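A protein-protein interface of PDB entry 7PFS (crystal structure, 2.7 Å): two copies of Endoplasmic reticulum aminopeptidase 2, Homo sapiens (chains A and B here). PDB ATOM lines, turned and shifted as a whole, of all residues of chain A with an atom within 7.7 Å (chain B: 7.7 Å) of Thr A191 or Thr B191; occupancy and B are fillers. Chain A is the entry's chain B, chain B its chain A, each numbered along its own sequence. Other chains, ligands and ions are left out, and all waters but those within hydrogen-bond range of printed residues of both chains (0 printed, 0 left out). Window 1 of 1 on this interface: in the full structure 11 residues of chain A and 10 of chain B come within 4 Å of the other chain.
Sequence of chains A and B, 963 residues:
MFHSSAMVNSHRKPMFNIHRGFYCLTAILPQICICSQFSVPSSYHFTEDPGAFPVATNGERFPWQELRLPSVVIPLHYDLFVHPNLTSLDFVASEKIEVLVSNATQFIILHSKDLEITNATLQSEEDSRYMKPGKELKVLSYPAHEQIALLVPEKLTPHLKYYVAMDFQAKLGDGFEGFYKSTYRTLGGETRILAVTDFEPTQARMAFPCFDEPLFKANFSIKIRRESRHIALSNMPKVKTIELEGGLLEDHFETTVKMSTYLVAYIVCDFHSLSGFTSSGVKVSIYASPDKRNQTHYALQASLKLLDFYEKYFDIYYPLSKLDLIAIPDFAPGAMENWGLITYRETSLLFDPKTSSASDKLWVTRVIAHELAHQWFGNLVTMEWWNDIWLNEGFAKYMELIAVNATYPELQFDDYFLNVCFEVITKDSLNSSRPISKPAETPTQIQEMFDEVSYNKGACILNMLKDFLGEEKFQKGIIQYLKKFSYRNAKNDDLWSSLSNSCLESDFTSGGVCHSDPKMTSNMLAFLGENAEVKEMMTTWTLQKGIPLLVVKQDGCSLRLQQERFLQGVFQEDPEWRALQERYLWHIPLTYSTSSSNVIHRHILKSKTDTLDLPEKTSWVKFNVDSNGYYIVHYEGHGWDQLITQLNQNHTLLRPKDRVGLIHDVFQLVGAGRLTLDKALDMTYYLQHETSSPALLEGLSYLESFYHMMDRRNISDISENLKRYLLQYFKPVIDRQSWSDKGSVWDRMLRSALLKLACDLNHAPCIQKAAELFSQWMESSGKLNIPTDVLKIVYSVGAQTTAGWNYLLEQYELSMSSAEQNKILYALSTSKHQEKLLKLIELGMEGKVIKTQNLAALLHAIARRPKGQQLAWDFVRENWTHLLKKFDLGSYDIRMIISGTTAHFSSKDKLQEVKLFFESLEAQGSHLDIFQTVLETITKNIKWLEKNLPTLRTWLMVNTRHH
Gly A189 touches Thr B191, and with the chains exchanged Thr A191 touches Gly B189. Glu A190 touches Thr B191, and with the chains exchanged Thr A191 touches Glu B190. Thr A191 touches its own counterpart, Thr B191. Arg A192 touches Arg B229, and with the chains exchanged Arg A229 touches Arg B192. Positions printed for both chains: 182, 183, 184, 185, 186, 188, 189, 190, 191, 192, 193 and 229.
Of the 12 printed residues of chain A, 7 touch a printed residue of chain B. Hydrophobic or aromatic side chains of chain A that line the printed part of chain B: Ile A193. Of the 12 printed residues of chain B, 7 touch a printed residue of chain A. Printed residues of chain B that touch a printed residue of chain A: Gly B188, Gly B189, Glu B190, Thr B191, Arg B192, Ile B193 and Arg B229. Among the printed residues, 15 pairs touch across the chains. Among the printed residues, Asp or Glu carboxylates within 4 Å of a Lys or Arg side-chain nitrogen of the other chain: Glu A190 with Arg B229 (2.7 Å) and Arg A229 with Glu B190 (3.4 Å).
OE2 of Glu B190 lies within salt-bridge range of NH1 of Arg A229 (3.4 Å). The backbone carbonyl oxygen (O) of Gly B189 lies within hydrogen-bond range of the side-chain hydroxyl (OG1) of Thr A191 (3.4 Å). The guanidinium group (NH2) of Arg B192 sits close to the guanidinium group (NH1) of Arg A229 (3.0 Å). O of Thr A191 sits at hydrogen-bond distance from N of Thr B191 (3.0 Å). OE2 of Glu A190 lies within salt-bridge range of NH1 of Arg B229.
Among the printed residues, merely in contact across the chains: Gly A188 with Ile B193, Gly A189 with Thr B191, Glu A190 with Thr B191, Glu A190 with Arg B192, Glu A190 with Ile B193, Thr A191 with Glu B190, Arg A192 with Glu B190, Arg A192 with Arg B229, Ile A193 with Gly B188 and Ile A193 with Glu B190.
Thr A186 touches none of the printed residues of chain B. Printed residues of chain B within 4 Å of Gly A188: Ile B193 (2.9 Å). Of the printed residues of chain B, Glu A190 touches Thr B191, Arg B192, Ile B193 and Arg B229. Thr A191 touches just these residues of chain B: Gly B189 (3.4 Å), Glu B190 (3.0 Å) and Thr B191 (3.0 Å). Of the printed residues of chain B, Ile A193 touches Gly B188 and Glu B190. Ser B182 touches none of the printed residues of chain A. Of the printed residues of chain A, Glu B190 touches Thr A191, Arg A192, Ile A193 and Arg A229. Thr B191 touches three residues of chain A. Of the printed residues of chain A, Arg B229 touches Glu A190 (2.7 Å) and Arg A192 (3.6 Å). The nearest residue of chain B that does not touch Thr A191 is Arg B192 (5.2 Å).
The backbone carbonyl oxygen (O) of Arg A192 sits at hydrogen-bond distance from the backbone NH (N) of Tyr A184, at 3.0 Å. The side-chain hydroxyl (OG1) of Thr B186 lies within hydrogen-bond range of the backbone NH (N) of Gly B188, 3.1 Å away. OG1 of Thr B186 lies within hydrogen-bond range of N of Glu B190 (3.1 Å). OE2 of Glu B190 is in salt-bridge range of NH2 of Arg B192. The backbone carbonyl oxygen (O) of Glu A190 sits at hydrogen-bond distance from the side-chain hydroxyl (OG1) of Thr A186. O of Tyr B184 lies within hydrogen-bond range of N of Arg B192 (3.0 Å).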
ATOM      1  N   SER A 182      -9.710 -19.479  -8.566  1.00  0.00           N
ATOM      2  CA  SER A 182      -9.063 -18.288  -8.047  1.00  0.00           C
ATOM      3  C   SER A 182      -9.523 -17.096  -8.881  1.00  0.00           C
ATOM      4  O   SER A 182      -9.822 -17.242 -10.074  1.00  0.00           O
ATOM      5  CB  SER A 182      -7.512 -18.410  -8.092  1.00  0.00           C
ATOM      6  OG  SER A 182      -6.888 -17.383  -7.334  1.00  0.00           O
ATOM      7  N   THR A 183      -9.563 -15.916  -8.256  1.00  0.00           N
ATOM      8  CA  THR A 183      -9.893 -14.674  -8.930  1.00  0.00           C
ATOM      9  C   THR A 183      -8.719 -13.715  -8.825  1.00  0.00           C
ATOM     10  O   THR A 183      -7.826 -13.890  -7.999  1.00  0.00           O
ATOM     11  CB  THR A 183     -11.159 -14.036  -8.331  1.00  0.00           C
ATOM     12  OG1 THR A 183     -12.076 -15.056  -7.930  1.00  0.00           O
ATOM     13  CG2 THR A 183     -11.881 -13.166  -9.389  1.00  0.00           C
ATOM     14  N   TYR A 184      -8.720 -12.706  -9.687  1.00  0.00           N
ATOM     15  CA  TYR A 184      -7.757 -11.626  -9.567  1.00  0.00           C
ATOM     16  C   TYR A 184      -8.378 -10.365 -10.137  1.00  0.00           C
ATOM     17  O   TYR A 184      -9.305 -10.425 -10.953  1.00  0.00           O
ATOM     18  CB  TYR A 184      -6.424 -11.931 -10.271  1.00  0.00           C
ATOM     19  CG  TYR A 184      -6.473 -12.033 -11.773  1.00  0.00           C
ATOM     20  CD1 TYR A 184      -6.196 -10.922 -12.573  1.00  0.00           C
ATOM     21  CD2 TYR A 184      -6.805 -13.241 -12.401  1.00  0.00           C
ATOM     22  CE1 TYR A 184      -6.220 -11.012 -13.990  1.00  0.00           C
ATOM     23  CE2 TYR A 184      -6.864 -13.341 -13.784  1.00  0.00           C
ATOM     24  CZ  TYR A 184      -6.562 -12.226 -14.591  1.00  0.00           C
ATOM     25  OH  TYR A 184      -6.603 -12.334 -15.990  1.00  0.00           O
ATOM     26  N   ARG A 185      -7.859  -9.219  -9.678  1.00  0.00           N
ATOM     27  CA  ARG A 185      -8.298  -7.905 -10.127  1.00  0.00           C
ATOM     28  C   ARG A 185      -7.371  -7.399 -11.221  1.00  0.00           C
ATOM     29  O   ARG A 185      -6.212  -7.802 -11.308  1.00  0.00           O
ATOM     30  CB  ARG A 185      -8.351  -6.894  -8.978  1.00  0.00           C
ATOM     31  CG  ARG A 185      -9.515  -5.918  -9.103  1.00  0.00           C
ATOM     32  CD  ARG A 185      -9.295  -4.640  -8.297  1.00  0.00           C
ATOM     33  NE  ARG A 185      -8.398  -3.703  -8.979  1.00  0.00           N
ATOM     34  CZ  ARG A 185      -8.488  -2.379  -8.890  1.00  0.00           C
ATOM     35  NH1 ARG A 185      -9.437  -1.828  -8.139  1.00  0.00           N
ATOM     36  NH2 ARG A 185      -7.632  -1.606  -9.554  1.00  0.00           N
ATOM     37  N   THR A 186      -7.907  -6.547 -12.087  1.00  0.00           N
ATOM     38  CA  THR A 186      -7.118  -5.979 -13.162  1.00  0.00           C
ATOM     39  C   THR A 186      -6.970  -4.485 -12.935  1.00  0.00           C
ATOM     40  O   THR A 186      -7.462  -3.938 -11.940  1.00  0.00           O
ATOM     41  CB  THR A 186      -7.770  -6.243 -14.510  1.00  0.00           C
ATOM     42  OG1 THR A 186      -9.046  -5.590 -14.543  1.00  0.00           O
ATOM     43  CG2 THR A 186      -7.922  -7.730 -14.760  1.00  0.00           C
ATOM     44  N   GLY A 188      -8.337  -1.953 -14.649  1.00  0.00           N
ATOM     45  CA  GLY A 188      -9.633  -1.317 -14.656  1.00  0.00           C
ATOM     46  C   GLY A 188     -10.625  -1.823 -13.632  1.00  0.00           C
ATOM     47  O   GLY A 188     -11.762  -1.336 -13.555  1.00  0.00           O
ATOM     48  N   GLY A 189     -10.231  -2.785 -12.811  1.00  0.00           N
ATOM     49  CA  GLY A 189     -11.123  -3.281 -11.784  1.00  0.00           C
ATOM     50  C   GLY A 189     -12.086  -4.362 -12.236  1.00  0.00           C
ATOM     51  O   GLY A 189     -13.050  -4.664 -11.505  1.00  0.00           O
ATOM     52  N   GLU A 190     -11.879  -4.936 -13.426  1.00  0.00           N
ATOM     53  CA  GLU A 190     -12.508  -6.212 -13.742  1.00  0.00           C
ATOM     54  C   GLU A 190     -11.870  -7.317 -12.893  1.00  0.00           C
ATOM     55  O   GLU A 190     -10.672  -7.282 -12.592  1.00  0.00           O
ATOM     56  CB  GLU A 190     -12.353  -6.568 -15.225  1.00  0.00           C
ATOM     57  CG  GLU A 190     -12.540  -5.450 -16.221  1.00  0.00           C
ATOM     58  CD  GLU A 190     -12.736  -5.972 -17.638  1.00  0.00           C
ATOM     59  OE1 GLU A 190     -13.512  -6.941 -17.809  1.00  0.00           O
ATOM     60  OE2 GLU A 190     -12.110  -5.414 -18.572  1.00  0.00           O
ATOM     61  N   THR A 191     -12.674  -8.310 -12.514  1.00  0.00           N
ATOM     62  CA  THR A 191     -12.129  -9.494 -11.873  1.00  0.00           C
ATOM     63  C   THR A 191     -12.307 -10.691 -12.800  1.00  0.00           C
ATOM     64  O   THR A 191     -13.396 -10.909 -13.336  1.00  0.00           O
ATOM     65  CB  THR A 191     -12.767  -9.750 -10.508  1.00  0.00           C
ATOM     66  OG1 THR A 191     -13.983 -10.485 -10.649  1.00  0.00           O
ATOM     67  CG2 THR A 191     -13.045  -8.444  -9.821  1.00  0.00           C
ATOM     68  N   ARG A 192     -11.219 -11.436 -13.008  1.00  0.00           N
ATOM     69  CA  ARG A 192     -11.244 -12.607 -13.858  1.00  0.00           C
ATOM     70  C   ARG A 192     -10.857 -13.842 -13.063  1.00  0.00           C
ATOM     71  O   ARG A 192     -10.279 -13.755 -11.977  1.00  0.00           O
ATOM     72  CB  ARG A 192     -10.345 -12.397 -15.064  1.00  0.00           C
ATOM     73  CG  ARG A 192     -10.807 -11.194 -15.859  1.00  0.00           C
ATOM     74  CD  ARG A 192     -10.003 -11.077 -17.096  1.00  0.00           C
ATOM     75  NE  ARG A 192      -9.871  -9.696 -17.515  1.00  0.00           N
ATOM     76  CZ  ARG A 192      -9.315  -9.346 -18.664  1.00  0.00           C
ATOM     77  NH1 ARG A 192      -8.863 -10.291 -19.487  1.00  0.00           N
ATOM     78  NH2 ARG A 192      -9.219  -8.067 -18.991  1.00  0.00           N
ATOM     79  N   ILE A 193     -11.194 -14.995 -13.625  1.00  0.00           N
ATOM     80  CA  ILE A 193     -11.242 -16.250 -12.897  1.00  0.00           C
ATOM     81  C   ILE A 193     -10.241 -17.197 -13.514  1.00  0.00           C
ATOM     82  O   ILE A 193     -10.059 -17.214 -14.738  1.00  0.00           O
ATOM     83  CB  ILE A 193     -12.660 -16.852 -12.936  1.00  0.00           C
ATOM     84  CG1 ILE A 193     -13.579 -16.018 -12.064  1.00  0.00           C
ATOM     85  CG2 ILE A 193     -12.702 -18.284 -12.412  1.00  0.00           C
ATOM     86  CD1 ILE A 193     -14.762 -16.785 -11.579  1.00  0.00           C
ATOM     87  N   ARG A 229     -10.844 -17.784 -25.190  1.00  0.00           N
ATOM     88  CA  ARG A 229     -10.279 -16.676 -24.449  1.00  0.00           C
ATOM     89  C   ARG A 229      -9.325 -17.106 -23.336  1.00  0.00           C
ATOM     90  O   ARG A 229      -8.858 -16.251 -22.573  1.00  0.00           O
ATOM     91  CB  ARG A 229     -11.405 -15.845 -23.847  1.00  0.00           C
ATOM     92  CG  ARG A 229     -11.938 -16.413 -22.586  1.00  0.00           C
ATOM     93  CD  ARG A 229     -13.000 -15.569 -21.944  1.00  0.00           C
ATOM     94  NE  ARG A 229     -13.952 -16.467 -21.293  1.00  0.00           N
ATOM     95  CZ  ARG A 229     -14.323 -16.354 -20.025  1.00  0.00           C
ATOM     96  NH1 ARG A 229     -13.828 -15.351 -19.287  1.00  0.00           N
ATOM     97  NH2 ARG A 229     -15.183 -17.234 -19.505  1.00  0.00           N
ATOM     98  N   SER B 182     -19.573   1.551 -16.367  1.00  0.00           N
ATOM     99  CA  SER B 182     -20.533   0.724 -15.658  1.00  0.00           C
ATOM    100  C   SER B 182     -19.929  -0.664 -15.556  1.00  0.00           C
ATOM    101  O   SER B 182     -19.068  -1.036 -16.357  1.00  0.00           O
ATOM    102  CB  SER B 182     -21.892   0.677 -16.395  1.00  0.00           C
ATOM    103  OG  SER B 182     -22.861  -0.112 -15.735  1.00  0.00           O
ATOM    104  N   THR B 183     -20.395  -1.450 -14.593  1.00  0.00           N
ATOM    105  CA  THR B 183     -19.868  -2.797 -14.425  1.00  0.00           C
ATOM    106  C   THR B 183     -21.000  -3.777 -14.174  1.00  0.00           C
ATOM    107  O   THR B 183     -22.067  -3.416 -13.671  1.00  0.00           O
ATOM    108  CB  THR B 183     -18.882  -2.864 -13.263  1.00  0.00           C
ATOM    109  OG1 THR B 183     -19.509  -2.333 -12.068  1.00  0.00           O
ATOM    110  CG2 THR B 183     -17.620  -2.081 -13.616  1.00  0.00           C
ATOM    111  N   TYR B 184     -20.747  -5.033 -14.489  1.00  0.00           N
ATOM    112  CA  TYR B 184     -21.679  -6.072 -14.092  1.00  0.00           C
ATOM    113  C   TYR B 184     -20.937  -7.329 -13.636  1.00  0.00           C
ATOM    114  O   TYR B 184     -19.720  -7.494 -13.847  1.00  0.00           O
ATOM    115  CB  TYR B 184     -22.608  -6.404 -15.226  1.00  0.00           C
ATOM    116  CG  TYR B 184     -21.924  -7.067 -16.400  1.00  0.00           C
ATOM    117  CD1 TYR B 184     -21.195  -6.323 -17.332  1.00  0.00           C
ATOM    118  CD2 TYR B 184     -22.054  -8.433 -16.608  1.00  0.00           C
ATOM    119  CE1 TYR B 184     -20.618  -6.935 -18.451  1.00  0.00           C
ATOM    120  CE2 TYR B 184     -21.488  -9.055 -17.712  1.00  0.00           C
ATOM    121  CZ  TYR B 184     -20.771  -8.302 -18.633  1.00  0.00           C
ATOM    122  OH  TYR B 184     -20.193  -8.934 -19.718  1.00  0.00           O
ATOM    123  N   ARG B 185     -21.706  -8.237 -13.026  1.00  0.00           N
ATOM    124  CA  ARG B 185     -21.189  -9.518 -12.562  1.00  0.00           C
ATOM    125  C   ARG B 185     -21.712 -10.645 -13.450  1.00  0.00           C
ATOM    126  O   ARG B 185     -22.869 -10.632 -13.878  1.00  0.00           O
ATOM    127  CB  ARG B 185     -21.558  -9.772 -11.092  1.00  0.00           C
ATOM    128  CG  ARG B 185     -20.797 -10.931 -10.446  1.00  0.00           C
ATOM    129  CD  ARG B 185     -21.298 -11.276  -9.031  1.00  0.00           C
ATOM    130  NE  ARG B 185     -22.258 -12.383  -9.067  1.00  0.00           N
ATOM    131  CZ  ARG B 185     -22.044 -13.605  -8.572  1.00  0.00           C
ATOM    132  NH1 ARG B 185     -20.894 -13.904  -7.968  1.00  0.00           N
ATOM    133  NH2 ARG B 185     -22.994 -14.530  -8.682  1.00  0.00           N
ATOM    134  N   THR B 186     -20.846 -11.611 -13.737  1.00  0.00           N
ATOM    135  CA  THR B 186     -21.198 -12.759 -14.555  1.00  0.00           C
ATOM    136  C   THR B 186     -21.659 -13.906 -13.672  1.00  0.00           C
ATOM    137  O   THR B 186     -21.723 -13.786 -12.442  1.00  0.00           O
ATOM    138  CB  THR B 186     -20.005 -13.219 -15.377  1.00  0.00           C
ATOM    139  OG1 THR B 186     -19.053 -13.867 -14.503  1.00  0.00           O
ATOM    140  CG2 THR B 186     -19.369 -12.016 -16.124  1.00  0.00           C
ATOM    141  N   GLY B 188     -19.880 -16.645 -13.322  1.00  0.00           N
ATOM    142  CA  GLY B 188     -18.686 -17.119 -12.644  1.00  0.00           C
ATOM    143  C   GLY B 188     -18.261 -16.256 -11.485  1.00  0.00           C
ATOM    144  O   GLY B 188     -17.464 -16.694 -10.656  1.00  0.00           O
ATOM    145  N   GLY B 189     -18.806 -15.058 -11.381  1.00  0.00           N
ATOM    146  CA  GLY B 189     -18.379 -14.112 -10.381  1.00  0.00           C
ATOM    147  C   GLY B 189     -17.393 -13.096 -10.911  1.00  0.00           C
ATOM    148  O   GLY B 189     -16.896 -12.259 -10.137  1.00  0.00           O
ATOM    149  N   GLU B 190     -17.096 -13.139 -12.204  1.00  0.00           N
ATOM    150  CA  GLU B 190     -16.230 -12.133 -12.790  1.00  0.00           C
ATOM    151  C   GLU B 190     -16.947 -10.778 -12.827  1.00  0.00           C
ATOM    152  O   GLU B 190     -18.186 -10.688 -12.803  1.00  0.00           O
ATOM    153  CB  GLU B 190     -15.785 -12.575 -14.189  1.00  0.00           C
ATOM    154  CG  GLU B 190     -14.880 -13.813 -14.163  1.00  0.00           C
ATOM    155  CD  GLU B 190     -14.528 -14.359 -15.541  1.00  0.00           C
ATOM    156  OE1 GLU B 190     -15.035 -15.455 -15.894  1.00  0.00           O
ATOM    157  OE2 GLU B 190     -13.737 -13.708 -16.264  1.00  0.00           O
ATOM    158  N   THR B 191     -16.142  -9.719 -12.853  1.00  0.00           N
ATOM    159  CA  THR B 191     -16.603  -8.347 -13.009  1.00  0.00           C
ATOM    160  C   THR B 191     -16.140  -7.818 -14.361  1.00  0.00           C
ATOM    161  O   THR B 191     -14.964  -7.944 -14.709  1.00  0.00           O
ATOM    162  CB  THR B 191     -16.059  -7.473 -11.878  1.00  0.00           C
ATOM    163  OG1 THR B 191     -16.477  -8.020 -10.615  1.00  0.00           O
ATOM    164  CG2 THR B 191     -16.554  -6.028 -12.034  1.00  0.00           C
ATOM    165  N   ARG B 192     -17.067  -7.254 -15.133  1.00  0.00           N
ATOM    166  CA  ARG B 192     -16.764  -6.713 -16.449  1.00  0.00           C
ATOM    167  C   ARG B 192     -17.177  -5.250 -16.530  1.00  0.00           C
ATOM    168  O   ARG B 192     -18.100  -4.793 -15.839  1.00  0.00           O
ATOM    169  CB  ARG B 192     -17.470  -7.506 -17.556  1.00  0.00           C
ATOM    170  CG  ARG B 192     -17.182  -8.984 -17.515  1.00  0.00           C
ATOM    171  CD  ARG B 192     -16.387  -9.451 -18.717  1.00  0.00           C
ATOM    172  NE  ARG B 192     -15.601 -10.648 -18.430  1.00  0.00           N
ATOM    173  CZ  ARG B 192     -16.063 -11.897 -18.526  1.00  0.00           C
ATOM    174  NH1 ARG B 192     -17.320 -12.132 -18.899  1.00  0.00           N
ATOM    175  NH2 ARG B 192     -15.258 -12.913 -18.242  1.00  0.00           N
ATOM    176  N   ILE B 193     -16.486  -4.520 -17.380  1.00  0.00           N
ATOM    177  CA  ILE B 193     -16.689  -3.089 -17.518  1.00  0.00           C
ATOM    178  C   ILE B 193     -17.376  -2.858 -18.845  1.00  0.00           C
ATOM    179  O   ILE B 193     -17.163  -3.609 -19.807  1.00  0.00           O
ATOM    180  CB  ILE B 193     -15.349  -2.314 -17.437  1.00  0.00           C
ATOM    181  CG1 ILE B 193     -14.616  -2.690 -16.156  1.00  0.00           C
ATOM    182  CG2 ILE B 193     -15.577  -0.837 -17.391  1.00  0.00           C
ATOM    183  CD1 ILE B 193     -13.325  -1.923 -15.957  1.00  0.00           C
ATOM    184  N   ARG B 229     -11.929  -7.880 -27.909  1.00  0.00           N
ATOM    185  CA  ARG B 229     -12.907  -8.525 -27.048  1.00  0.00           C
ATOM    186  C   ARG B 229     -14.216  -7.755 -26.913  1.00  0.00           C
ATOM    187  O   ARG B 229     -15.165  -8.307 -26.336  1.00  0.00           O
ATOM    188  CB  ARG B 229     -12.320  -8.745 -25.649  1.00  0.00           C
ATOM    189  CG  ARG B 229     -11.585  -7.531 -25.093  1.00  0.00           C
ATOM    190  CD  ARG B 229     -11.422  -7.523 -23.564  1.00  0.00           C
ATOM    191  NE  ARG B 229     -10.711  -6.315 -23.136  1.00  0.00           N
ATOM    192  CZ  ARG B 229     -10.852  -5.769 -21.930  1.00  0.00           C
ATOM    193  NH1 ARG B 229     -11.655  -6.346 -21.038  1.00  0.00           N
ATOM    194  NH2 ARG B 229     -10.184  -4.665 -21.598  1.00  0.00           N
